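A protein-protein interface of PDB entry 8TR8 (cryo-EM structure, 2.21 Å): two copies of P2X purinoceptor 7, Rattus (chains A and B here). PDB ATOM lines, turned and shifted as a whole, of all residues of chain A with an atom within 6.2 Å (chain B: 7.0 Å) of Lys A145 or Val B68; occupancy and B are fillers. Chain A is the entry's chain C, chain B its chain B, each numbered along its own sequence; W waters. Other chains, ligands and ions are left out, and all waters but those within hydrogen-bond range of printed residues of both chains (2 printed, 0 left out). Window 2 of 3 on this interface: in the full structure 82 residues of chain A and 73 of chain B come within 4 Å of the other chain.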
ATOM      1  N   MET A 140       9.125 -17.781   0.221  1.00  0.00           N
ATOM      2  CA  MET A 140      10.336 -17.478   0.962  1.00  0.00           C
ATOM      3  C   MET A 140      11.504 -18.277   0.409  1.00  0.00           C
ATOM      4  O   MET A 140      11.441 -19.506   0.318  1.00  0.00           O
ATOM      5  CB  MET A 140      10.135 -17.792   2.442  1.00  0.00           C
ATOM      6  CG  MET A 140      11.171 -17.185   3.348  1.00  0.00           C
ATOM      7  SD  MET A 140      12.738 -18.076   3.356  1.00  0.00           S
ATOM      8  CE  MET A 140      12.236 -19.615   4.102  1.00  0.00           C
ATOM      9  N   ASP A 141      12.571 -17.578   0.044  1.00  0.00           N
ATOM     10  CA  ASP A 141      13.800 -18.227  -0.390  1.00  0.00           C
ATOM     11  C   ASP A 141      14.817 -18.152   0.737  1.00  0.00           C
ATOM     12  O   ASP A 141      15.335 -17.062   1.022  1.00  0.00           O
ATOM     13  CB  ASP A 141      14.350 -17.565  -1.655  1.00  0.00           C
ATOM     14  CG  ASP A 141      15.378 -18.423  -2.359  1.00  0.00           C
ATOM     15  OD1 ASP A 141      15.859 -19.399  -1.748  1.00  0.00           O
ATOM     16  OD2 ASP A 141      15.706 -18.123  -3.526  1.00  0.00           O
ATOM     17  N   PRO A 142      15.125 -19.259   1.420  1.00  0.00           N
ATOM     18  CA  PRO A 142      16.142 -19.203   2.479  1.00  0.00           C
ATOM     19  C   PRO A 142      17.539 -18.917   1.957  1.00  0.00           C
ATOM     20  O   PRO A 142      18.410 -18.545   2.751  1.00  0.00           O
ATOM     21  CB  PRO A 142      16.053 -20.589   3.128  1.00  0.00           C
ATOM     22  CG  PRO A 142      15.468 -21.461   2.085  1.00  0.00           C
ATOM     23  CD  PRO A 142      14.555 -20.609   1.276  1.00  0.00           C
ATOM     24  N   GLN A 143      17.778 -19.077   0.656  1.00  0.00           N
ATOM     25  CA  GLN A 143      19.096 -18.819   0.088  1.00  0.00           C
ATOM     26  C   GLN A 143      19.300 -17.330  -0.165  1.00  0.00           C
ATOM     27  O   GLN A 143      20.235 -16.719   0.361  1.00  0.00           O
ATOM     28  CB  GLN A 143      19.273 -19.617  -1.204  1.00  0.00           C
ATOM     29  N   SER A 144      18.431 -16.731  -0.978  1.00  0.00           N
ATOM     30  CA  SER A 144      18.473 -15.294  -1.195  1.00  0.00           C
ATOM     31  C   SER A 144      18.071 -14.517   0.047  1.00  0.00           C
ATOM     32  O   SER A 144      18.410 -13.337   0.166  1.00  0.00           O
ATOM     33  CB  SER A 144      17.557 -14.919  -2.356  1.00  0.00           C
ATOM     34  OG  SER A 144      16.213 -14.831  -1.928  1.00  0.00           O
ATOM     35  N   LYS A 145      17.353 -15.158   0.965  1.00  0.00           N
ATOM     36  CA  LYS A 145      16.951 -14.550   2.228  1.00  0.00           C
ATOM     37  C   LYS A 145      15.987 -13.392   1.993  1.00  0.00           C
ATOM     38  O   LYS A 145      16.107 -12.323   2.591  1.00  0.00           O
ATOM     39  CB  LYS A 145      18.171 -14.114   3.038  1.00  0.00           C
ATOM     40  CG  LYS A 145      19.110 -15.253   3.292  1.00  0.00           C
ATOM     41  CD  LYS A 145      20.135 -14.942   4.333  1.00  0.00           C
ATOM     42  CE  LYS A 145      20.944 -16.175   4.656  1.00  0.00           C
ATOM     43  NZ  LYS A 145      21.510 -16.780   3.443  1.00  0.00           N
ATOM     44  N   GLY A 146      15.013 -13.624   1.116  1.00  0.00           N
ATOM     45  CA  GLY A 146      13.996 -12.645   0.805  1.00  0.00           C
ATOM     46  C   GLY A 146      12.732 -13.325   0.332  1.00  0.00           C
ATOM     47  O   GLY A 146      12.697 -14.537   0.112  1.00  0.00           O
ATOM     48  N   ILE A 147      11.687 -12.522   0.181  1.00  0.00           N
ATOM     49  CA  ILE A 147      10.386 -12.994  -0.281  1.00  0.00           C
ATOM     50  C   ILE A 147      10.194 -12.535  -1.717  1.00  0.00           C
ATOM     51  O   ILE A 147      10.243 -11.334  -2.007  1.00  0.00           O
ATOM     52  CB  ILE A 147       9.244 -12.484   0.610  1.00  0.00           C
ATOM     53  CG1 ILE A 147       9.624 -12.538   2.095  1.00  0.00           C
ATOM     54  CG2 ILE A 147       7.988 -13.287   0.333  1.00  0.00           C
ATOM     55  CD1 ILE A 147       9.810 -13.922   2.660  1.00  0.00           C
ATOM     56  N   ILE A 164      12.824  -9.689  -5.077  1.00  0.00           N
ATOM     57  CA  ILE A 164      12.564 -10.130  -3.715  1.00  0.00           C
ATOM     58  C   ILE A 164      12.466  -8.915  -2.808  1.00  0.00           C
ATOM     59  O   ILE A 164      13.128  -7.897  -3.027  1.00  0.00           O
ATOM     60  CB  ILE A 164      13.651 -11.102  -3.192  1.00  0.00           C
ATOM     61  CG1 ILE A 164      15.049 -10.507  -3.374  1.00  0.00           C
ATOM     62  CG2 ILE A 164      13.545 -12.445  -3.879  1.00  0.00           C
ATOM     63  CD1 ILE A 164      16.129 -11.249  -2.632  1.00  0.00           C
ATOM     64  N   PHE A 165      11.622  -9.025  -1.791  1.00  0.00           N
ATOM     65  CA  PHE A 165      11.626  -8.085  -0.681  1.00  0.00           C
ATOM     66  C   PHE A 165      12.611  -8.599   0.358  1.00  0.00           C
ATOM     67  O   PHE A 165      12.428  -9.687   0.910  1.00  0.00           O
ATOM     68  CB  PHE A 165      10.231  -7.921  -0.079  1.00  0.00           C
ATOM     69  CG  PHE A 165      10.184  -6.963   1.071  1.00  0.00           C
ATOM     70  CD1 PHE A 165      10.151  -5.603   0.851  1.00  0.00           C
ATOM     71  CD2 PHE A 165      10.185  -7.421   2.371  1.00  0.00           C
ATOM     72  CE1 PHE A 165      10.115  -4.723   1.900  1.00  0.00           C
ATOM     73  CE2 PHE A 165      10.147  -6.543   3.422  1.00  0.00           C
ATOM     74  CZ  PHE A 165      10.116  -5.191   3.188  1.00  0.00           C
ATOM     75  N   ALA A 166      13.656  -7.822   0.612  1.00  0.00           N
ATOM     76  CA  ALA A 166      14.767  -8.279   1.428  1.00  0.00           C
ATOM     77  C   ALA A 166      15.565  -7.067   1.877  1.00  0.00           C
ATOM     78  O   ALA A 166      15.247  -5.927   1.535  1.00  0.00           O
ATOM     79  CB  ALA A 166      15.644  -9.259   0.646  1.00  0.00           C
ATOM     80  N   TRP A 167      16.597  -7.325   2.670  1.00  0.00           N
ATOM     81  CA  TRP A 167      17.644  -6.336   2.867  1.00  0.00           C
ATOM     82  C   TRP A 167      18.356  -6.116   1.541  1.00  0.00           C
ATOM     83  O   TRP A 167      18.893  -7.057   0.951  1.00  0.00           O
ATOM     84  CB  TRP A 167      18.634  -6.801   3.933  1.00  0.00           C
ATOM     85  CG  TRP A 167      18.129  -6.786   5.332  1.00  0.00           C
ATOM     86  CD1 TRP A 167      17.696  -7.853   6.054  1.00  0.00           C
ATOM     87  CD2 TRP A 167      18.034  -5.655   6.197  1.00  0.00           C
ATOM     88  NE1 TRP A 167      17.329  -7.458   7.307  1.00  0.00           N
ATOM     89  CE2 TRP A 167      17.529  -6.111   7.424  1.00  0.00           C
ATOM     90  CE3 TRP A 167      18.321  -4.299   6.052  1.00  0.00           C
ATOM     91  CZ2 TRP A 167      17.299  -5.260   8.497  1.00  0.00           C
ATOM     92  CZ3 TRP A 167      18.096  -3.458   7.117  1.00  0.00           C
ATOM     93  CH2 TRP A 167      17.591  -3.939   8.322  1.00  0.00           C
ATOM     94  N   GLU A 172      23.587 -12.103  -1.255  1.00  0.00           N
ATOM     95  CA  GLU A 172      23.677 -13.477  -0.790  1.00  0.00           C
ATOM     96  C   GLU A 172      23.812 -14.424  -1.973  1.00  0.00           C
ATOM     97  O   GLU A 172      23.046 -14.349  -2.937  1.00  0.00           O
ATOM     98  CB  GLU A 172      22.453 -13.829   0.052  1.00  0.00           C
ATOM     99  CG  GLU A 172      22.481 -13.272   1.469  1.00  0.00           C
ATOM    100  CD  GLU A 172      23.613 -13.828   2.308  1.00  0.00           C
ATOM    101  OE1 GLU A 172      23.761 -15.066   2.377  1.00  0.00           O
ATOM    102  OE2 GLU A 172      24.364 -13.021   2.897  1.00  0.00           O
ATOM    103  N   PHE A 288      26.051 -26.156   2.649  1.00  0.00           N
ATOM    104  CA  PHE A 288      26.832 -25.079   3.330  1.00  0.00           C
ATOM    105  C   PHE A 288      28.290 -25.517   3.527  1.00  0.00           C
ATOM    106  O   PHE A 288      28.753 -25.599   4.676  1.00  0.00           O
ATOM    107  CB  PHE A 288      26.215 -24.666   4.674  1.00  0.00           C
ATOM    108  CG  PHE A 288      24.805 -24.139   4.605  1.00  0.00           C
ATOM    109  CD1 PHE A 288      23.720 -24.997   4.668  1.00  0.00           C
ATOM    110  CD2 PHE A 288      24.568 -22.778   4.509  1.00  0.00           C
ATOM    111  CE1 PHE A 288      22.428 -24.504   4.615  1.00  0.00           C
ATOM    112  CE2 PHE A 288      23.273 -22.288   4.454  1.00  0.00           C
ATOM    113  CZ  PHE A 288      22.207 -23.151   4.507  1.00  0.00           C
ATOM    114  N   ARG A 294      26.890 -14.877   9.352  1.00  0.00           N
ATOM    115  CA  ARG A 294      26.450 -13.560   8.918  1.00  0.00           C
ATOM    116  C   ARG A 294      26.236 -12.684  10.145  1.00  0.00           C
ATOM    117  O   ARG A 294      25.433 -13.019  11.020  1.00  0.00           O
ATOM    118  CB  ARG A 294      25.175 -13.659   8.085  1.00  0.00           C
ATOM    119  CG  ARG A 294      25.370 -14.365   6.771  1.00  0.00           C
ATOM    120  CD  ARG A 294      24.064 -14.750   6.117  1.00  0.00           C
ATOM    121  NE  ARG A 294      23.425 -13.618   5.459  1.00  0.00           N
ATOM    122  CZ  ARG A 294      22.336 -12.995   5.891  1.00  0.00           C
ATOM    123  NH1 ARG A 294      21.718 -13.368   6.998  1.00  0.00           N
ATOM    124  NH2 ARG A 294      21.858 -11.982   5.196  1.00  0.00           N
ATOM    125  N   VAL B  65      20.977 -22.375  10.778  1.00  0.00           N
ATOM    126  CA  VAL B  65      19.549 -22.092  10.778  1.00  0.00           C
ATOM    127  C   VAL B  65      19.169 -21.454   9.448  1.00  0.00           C
ATOM    128  O   VAL B  65      19.868 -20.567   8.948  1.00  0.00           O
ATOM    129  CB  VAL B  65      19.167 -21.181  11.957  1.00  0.00           C
ATOM    130  CG1 VAL B  65      17.679 -20.855  11.933  1.00  0.00           C
ATOM    131  CG2 VAL B  65      19.552 -21.828  13.268  1.00  0.00           C
ATOM    132  N   LYS B  66      18.074 -21.924   8.869  1.00  0.00           N
ATOM    133  CA  LYS B  66      17.509 -21.371   7.649  1.00  0.00           C
ATOM    134  C   LYS B  66      16.122 -20.815   7.930  1.00  0.00           C
ATOM    135  O   LYS B  66      15.332 -21.429   8.652  1.00  0.00           O
ATOM    136  CB  LYS B  66      17.420 -22.421   6.536  1.00  0.00           C
ATOM    137  CG  LYS B  66      18.740 -22.904   5.982  1.00  0.00           C
ATOM    138  CD  LYS B  66      18.555 -24.119   5.080  1.00  0.00           C
ATOM    139  CE  LYS B  66      17.768 -23.787   3.831  1.00  0.00           C
ATOM    140  NZ  LYS B  66      17.538 -24.989   2.990  1.00  0.00           N
ATOM    141  N   GLY B  67      15.830 -19.653   7.359  1.00  0.00           N
ATOM    142  CA  GLY B  67      14.506 -19.081   7.475  1.00  0.00           C
ATOM    143  C   GLY B  67      14.428 -17.573   7.530  1.00  0.00           C
ATOM    144  O   GLY B  67      15.292 -16.903   8.098  1.00  0.00           O
ATOM    145  N   VAL B  68      13.369 -17.039   6.933  1.00  0.00           N
ATOM    146  CA  VAL B  68      13.064 -15.616   6.932  1.00  0.00           C
ATOM    147  C   VAL B  68      11.676 -15.444   7.527  1.00  0.00           C
ATOM    148  O   VAL B  68      10.733 -16.126   7.114  1.00  0.00           O
ATOM    149  CB  VAL B  68      13.123 -15.005   5.518  1.00  0.00           C
ATOM    150  CG1 VAL B  68      13.007 -13.496   5.568  1.00  0.00           C
ATOM    151  CG2 VAL B  68      14.378 -15.400   4.799  1.00  0.00           C
ATOM    152  N   ALA B  69      11.556 -14.543   8.488  1.00  0.00           N
ATOM    153  CA  ALA B  69      10.286 -14.255   9.135  1.00  0.00           C
ATOM    154  C   ALA B  69       9.696 -12.967   8.580  1.00  0.00           C
ATOM    155  O   ALA B  69      10.389 -11.953   8.481  1.00  0.00           O
ATOM    156  CB  ALA B  69      10.461 -14.146  10.646  1.00  0.00           C
ATOM    157  N   GLU B  70       8.418 -13.017   8.220  1.00  0.00           N
ATOM    158  CA  GLU B  70       7.651 -11.838   7.845  1.00  0.00           C
ATOM    159  C   GLU B  70       6.895 -11.331   9.061  1.00  0.00           C
ATOM    160  O   GLU B  70       6.235 -12.109   9.758  1.00  0.00           O
ATOM    161  CB  GLU B  70       6.662 -12.142   6.721  1.00  0.00           C
ATOM    162  CG  GLU B  70       7.038 -11.580   5.380  1.00  0.00           C
ATOM    163  CD  GLU B  70       5.889 -11.640   4.399  1.00  0.00           C
ATOM    164  OE1 GLU B  70       4.790 -12.079   4.783  1.00  0.00           O
ATOM    165  OE2 GLU B  70       6.085 -11.249   3.229  1.00  0.00           O
ATOM    166  N   GLY B  86       8.097  -5.760   7.475  1.00  0.00           N
ATOM    167  CA  GLY B  86       9.517  -6.031   7.497  1.00  0.00           C
ATOM    168  C   GLY B  86       9.787  -7.518   7.477  1.00  0.00           C
ATOM    169  O   GLY B  86       8.869  -8.337   7.525  1.00  0.00           O
ATOM    170  N   ILE B  87      11.072  -7.863   7.402  1.00  0.00           N
ATOM    171  CA  ILE B  87      11.513  -9.250   7.447  1.00  0.00           C
ATOM    172  C   ILE B  87      12.665  -9.388   8.433  1.00  0.00           C
ATOM    173  O   ILE B  87      13.368  -8.430   8.753  1.00  0.00           O
ATOM    174  CB  ILE B  87      11.933  -9.796   6.062  1.00  0.00           C
ATOM    175  CG1 ILE B  87      13.055  -8.957   5.445  1.00  0.00           C
ATOM    176  CG2 ILE B  87      10.748  -9.896   5.145  1.00  0.00           C
ATOM    177  CD1 ILE B  87      14.403  -9.602   5.540  1.00  0.00           C
ATOM    178  N   PHE B  88      12.841 -10.613   8.916  1.00  0.00           N
ATOM    179  CA  PHE B  88      13.944 -10.990   9.793  1.00  0.00           C
ATOM    180  C   PHE B  88      14.707 -12.126   9.132  1.00  0.00           C
ATOM    181  O   PHE B  88      14.138 -13.195   8.888  1.00  0.00           O
ATOM    182  CB  PHE B  88      13.446 -11.431  11.171  1.00  0.00           C
ATOM    183  CG  PHE B  88      13.121 -10.309  12.099  1.00  0.00           C
ATOM    184  CD1 PHE B  88      11.920  -9.640  12.007  1.00  0.00           C
ATOM    185  CD2 PHE B  88      14.008  -9.944  13.088  1.00  0.00           C
ATOM    186  CE1 PHE B  88      11.625  -8.622  12.867  1.00  0.00           C
ATOM    187  CE2 PHE B  88      13.708  -8.928  13.950  1.00  0.00           C
ATOM    188  CZ  PHE B  88      12.517  -8.266  13.839  1.00  0.00           C
ATOM    189  N   ASP B  89      15.980 -11.901   8.843  1.00  0.00           N
ATOM    190  CA  ASP B  89      16.853 -12.958   8.358  1.00  0.00           C
ATOM    191  C   ASP B  89      17.826 -13.370   9.463  1.00  0.00           C
ATOM    192  O   ASP B  89      17.838 -12.802  10.555  1.00  0.00           O
ATOM    193  CB  ASP B  89      17.560 -12.541   7.056  1.00  0.00           C
ATOM    194  CG  ASP B  89      18.647 -11.498   7.246  1.00  0.00           C
ATOM    195  OD1 ASP B  89      19.187 -11.323   8.354  1.00  0.00           O
ATOM    196  OD2 ASP B  89      18.983 -10.849   6.238  1.00  0.00           O
ATOM    197  N   THR B  90      18.638 -14.383   9.158  1.00  0.00           N
ATOM    198  CA  THR B  90      19.434 -15.062  10.177  1.00  0.00           C
ATOM    199  C   THR B  90      20.244 -14.091  11.026  1.00  0.00           C
ATOM    200  O   THR B  90      20.318 -14.245  12.249  1.00  0.00           O
ATOM    201  CB  THR B  90      20.355 -16.090   9.517  1.00  0.00           C
ATOM    202  OG1 THR B  90      21.026 -15.497   8.402  1.00  0.00           O
ATOM    203  CG2 THR B  90      19.562 -17.286   9.058  1.00  0.00           C
ATOM    204  N   ALA B  91      20.859 -13.088  10.400  1.00  0.00           N
ATOM    205  CA  ALA B  91      21.652 -12.122  11.150  1.00  0.00           C
ATOM    206  C   ALA B  91      20.796 -11.273  12.074  1.00  0.00           C
ATOM    207  O   ALA B  91      21.325 -10.681  13.021  1.00  0.00           O
ATOM    208  CB  ALA B  91      22.434 -11.232  10.186  1.00  0.00           C
ATOM    209  N   TYR B  93      18.290 -12.573  13.922  1.00  0.00           N
ATOM    210  CA  TYR B  93      17.740 -13.372  15.011  1.00  0.00           C
ATOM    211  C   TYR B  93      18.683 -14.447  15.552  1.00  0.00           C
ATOM    212  O   TYR B  93      18.257 -15.235  16.407  1.00  0.00           O
ATOM    213  CB  TYR B  93      16.405 -14.013  14.580  1.00  0.00           C
ATOM    214  CG  TYR B  93      16.466 -15.016  13.448  1.00  0.00           C
ATOM    215  CD1 TYR B  93      16.997 -16.275  13.642  1.00  0.00           C
ATOM    216  CD2 TYR B  93      15.942 -14.721  12.200  1.00  0.00           C
ATOM    217  CE1 TYR B  93      17.048 -17.184  12.638  1.00  0.00           C
ATOM    218  CE2 TYR B  93      15.984 -15.637  11.184  1.00  0.00           C
ATOM    219  CZ  TYR B  93      16.537 -16.872  11.409  1.00  0.00           C
ATOM    220  OH  TYR B  93      16.589 -17.807  10.413  1.00  0.00           O
ATOM    221  N   SER B 184       6.870 -16.841  14.168  1.00  0.00           N
ATOM    222  CA  SER B 184       6.998 -17.533  12.894  1.00  0.00           C
ATOM    223  C   SER B 184       8.300 -18.313  12.777  1.00  0.00           C
ATOM    224  O   SER B 184       8.496 -19.015  11.781  1.00  0.00           O
ATOM    225  CB  SER B 184       6.886 -16.530  11.751  1.00  0.00           C
ATOM    226  OG  SER B 184       7.805 -15.473  11.901  1.00  0.00           O
ATOM    227  N   ASN B 187       8.587 -22.148  11.903  1.00  0.00           N
ATOM    228  CA  ASN B 187       8.774 -22.631  10.548  1.00  0.00           C
ATOM    229  C   ASN B 187      10.228 -22.592  10.093  1.00  0.00           C
ATOM    230  O   ASN B 187      10.518 -23.023   8.973  1.00  0.00           O
ATOM    231  CB  ASN B 187       7.905 -21.816   9.589  1.00  0.00           C
ATOM    232  CG  ASN B 187       6.486 -22.336   9.490  1.00  0.00           C
ATOM    233  OD1 ASN B 187       6.220 -23.509   9.736  1.00  0.00           O
ATOM    234  ND2 ASN B 187       5.564 -21.457   9.122  1.00  0.00           N
ATOM    235  N   PHE B 188      11.145 -22.094  10.917  1.00  0.00           N
ATOM    236  CA  PHE B 188      12.558 -22.169  10.589  1.00  0.00           C
ATOM    237  C   PHE B 188      13.044 -23.614  10.644  1.00  0.00           C
ATOM    238  O   PHE B 188      12.465 -24.475  11.310  1.00  0.00           O
ATOM    239  CB  PHE B 188      13.405 -21.328  11.551  1.00  0.00           C
ATOM    240  CG  PHE B 188      13.145 -19.851  11.496  1.00  0.00           C
ATOM    241  CD1 PHE B 188      12.348 -19.290  10.523  1.00  0.00           C
ATOM    242  CD2 PHE B 188      13.710 -19.020  12.441  1.00  0.00           C
ATOM    243  CE1 PHE B 188      12.125 -17.945  10.502  1.00  0.00           C
ATOM    244  CE2 PHE B 188      13.483 -17.677  12.415  1.00  0.00           C
ATOM    245  CZ  PHE B 188      12.693 -17.139  11.443  1.00  0.00           C
HETATM  246  O   HOH W   1      17.493 -10.277   3.725  1.00  0.00           O
HETATM  247  O   HOH W   2      18.059 -18.399   5.771  1.00  0.00           O
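The side-chain carboxylate (OD2) of Asp B89 is in salt-bridge range of the guanidinium group (NH2) of Arg A294 (3.3 Å). OG1 of Thr B90 sits at hydrogen-bond distance from NH1 of Arg A294 (2.6 Å). SD of Met A140 sits close to N of Val B68, 3.8 Å away.
NE of Arg A294 is in salt-bridge range of OE2 of Glu A172. OD1 of Asp B89 sits at hydrogen-bond distance from N of Ala B91 (3.2 Å). The backbone carbonyl oxygen (O) of Gln A143 is in hydrogen-bond range of the side-chain amino group (NZ) of Lys A145 (3.3 Å). NZ of Lys A145 is in salt-bridge range of OE1 of Glu A172. The backbone NH of Phe A165 is in hydrogen-bond range of the backbone carbonyl oxygen of Ile A147, at 2.7 Å.
Pro A142 touches Lys B66. Lys A145 touches Val B68. Lys A145 touches Thr B90 (CE to OG1, 3.8 Å). OE2 of Glu B70 touches CG1 of Ile A147 (3.9 Å). Phe A165 touches Ile B87 (CD2 to CG2, 3.8 Å). CD1 of Trp A167 touches CD1 of Ile B87 (3.8 Å). Asp B89 touches Trp A167. Phe A288 touches Lys B66 (CZ to CG, 3.8 Å). Arg A294 touches Ala B91.
Of the printed residues of chain B, Pro A142 touches Lys B66 (3.7 Å). Of chain B, only Val B68 (3.7 Å) and Thr B90 (3.8 Å) come within 4 Å of Lys A145. Val B68 touches just these residues of chain A: Met A140 and Lys A145. Of the printed residues of chain A, Glu B70 touches Ile A147. Printed residues of chain A within 4 Å of Ala B91: Arg A294 (3.5 Å). The nearest printed residue of chain A that does not touch Lys B66 is Met A140 (5.6 Å).
Of the 16 printed residues of chain B, 7 touch a printed residue of chain A. Hydrophobic or aromatic side chains of chain B within 4 Å of the printed part of chain A: Val B68, Ile B87 and Ala B91. Of the 15 printed residues of chain A, 8 touch a printed residue of chain B. Among the printed residues, Asp or Glu carboxylates within 4 Å of a Lys or Arg side-chain nitrogen of the other chain: Arg A294 with Asp B89.
No position is printed for both chains.
Water W1 lies within hydrogen-bond range of O of Lys A145 (2.7 Å), OD2 of Asp B89 (3.0 Å) and N of Trp A167 (3.3 Å). Water W2 bridges N of Gly B67 (3.0 Å) and O of Pro A142 (3.0 Å).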
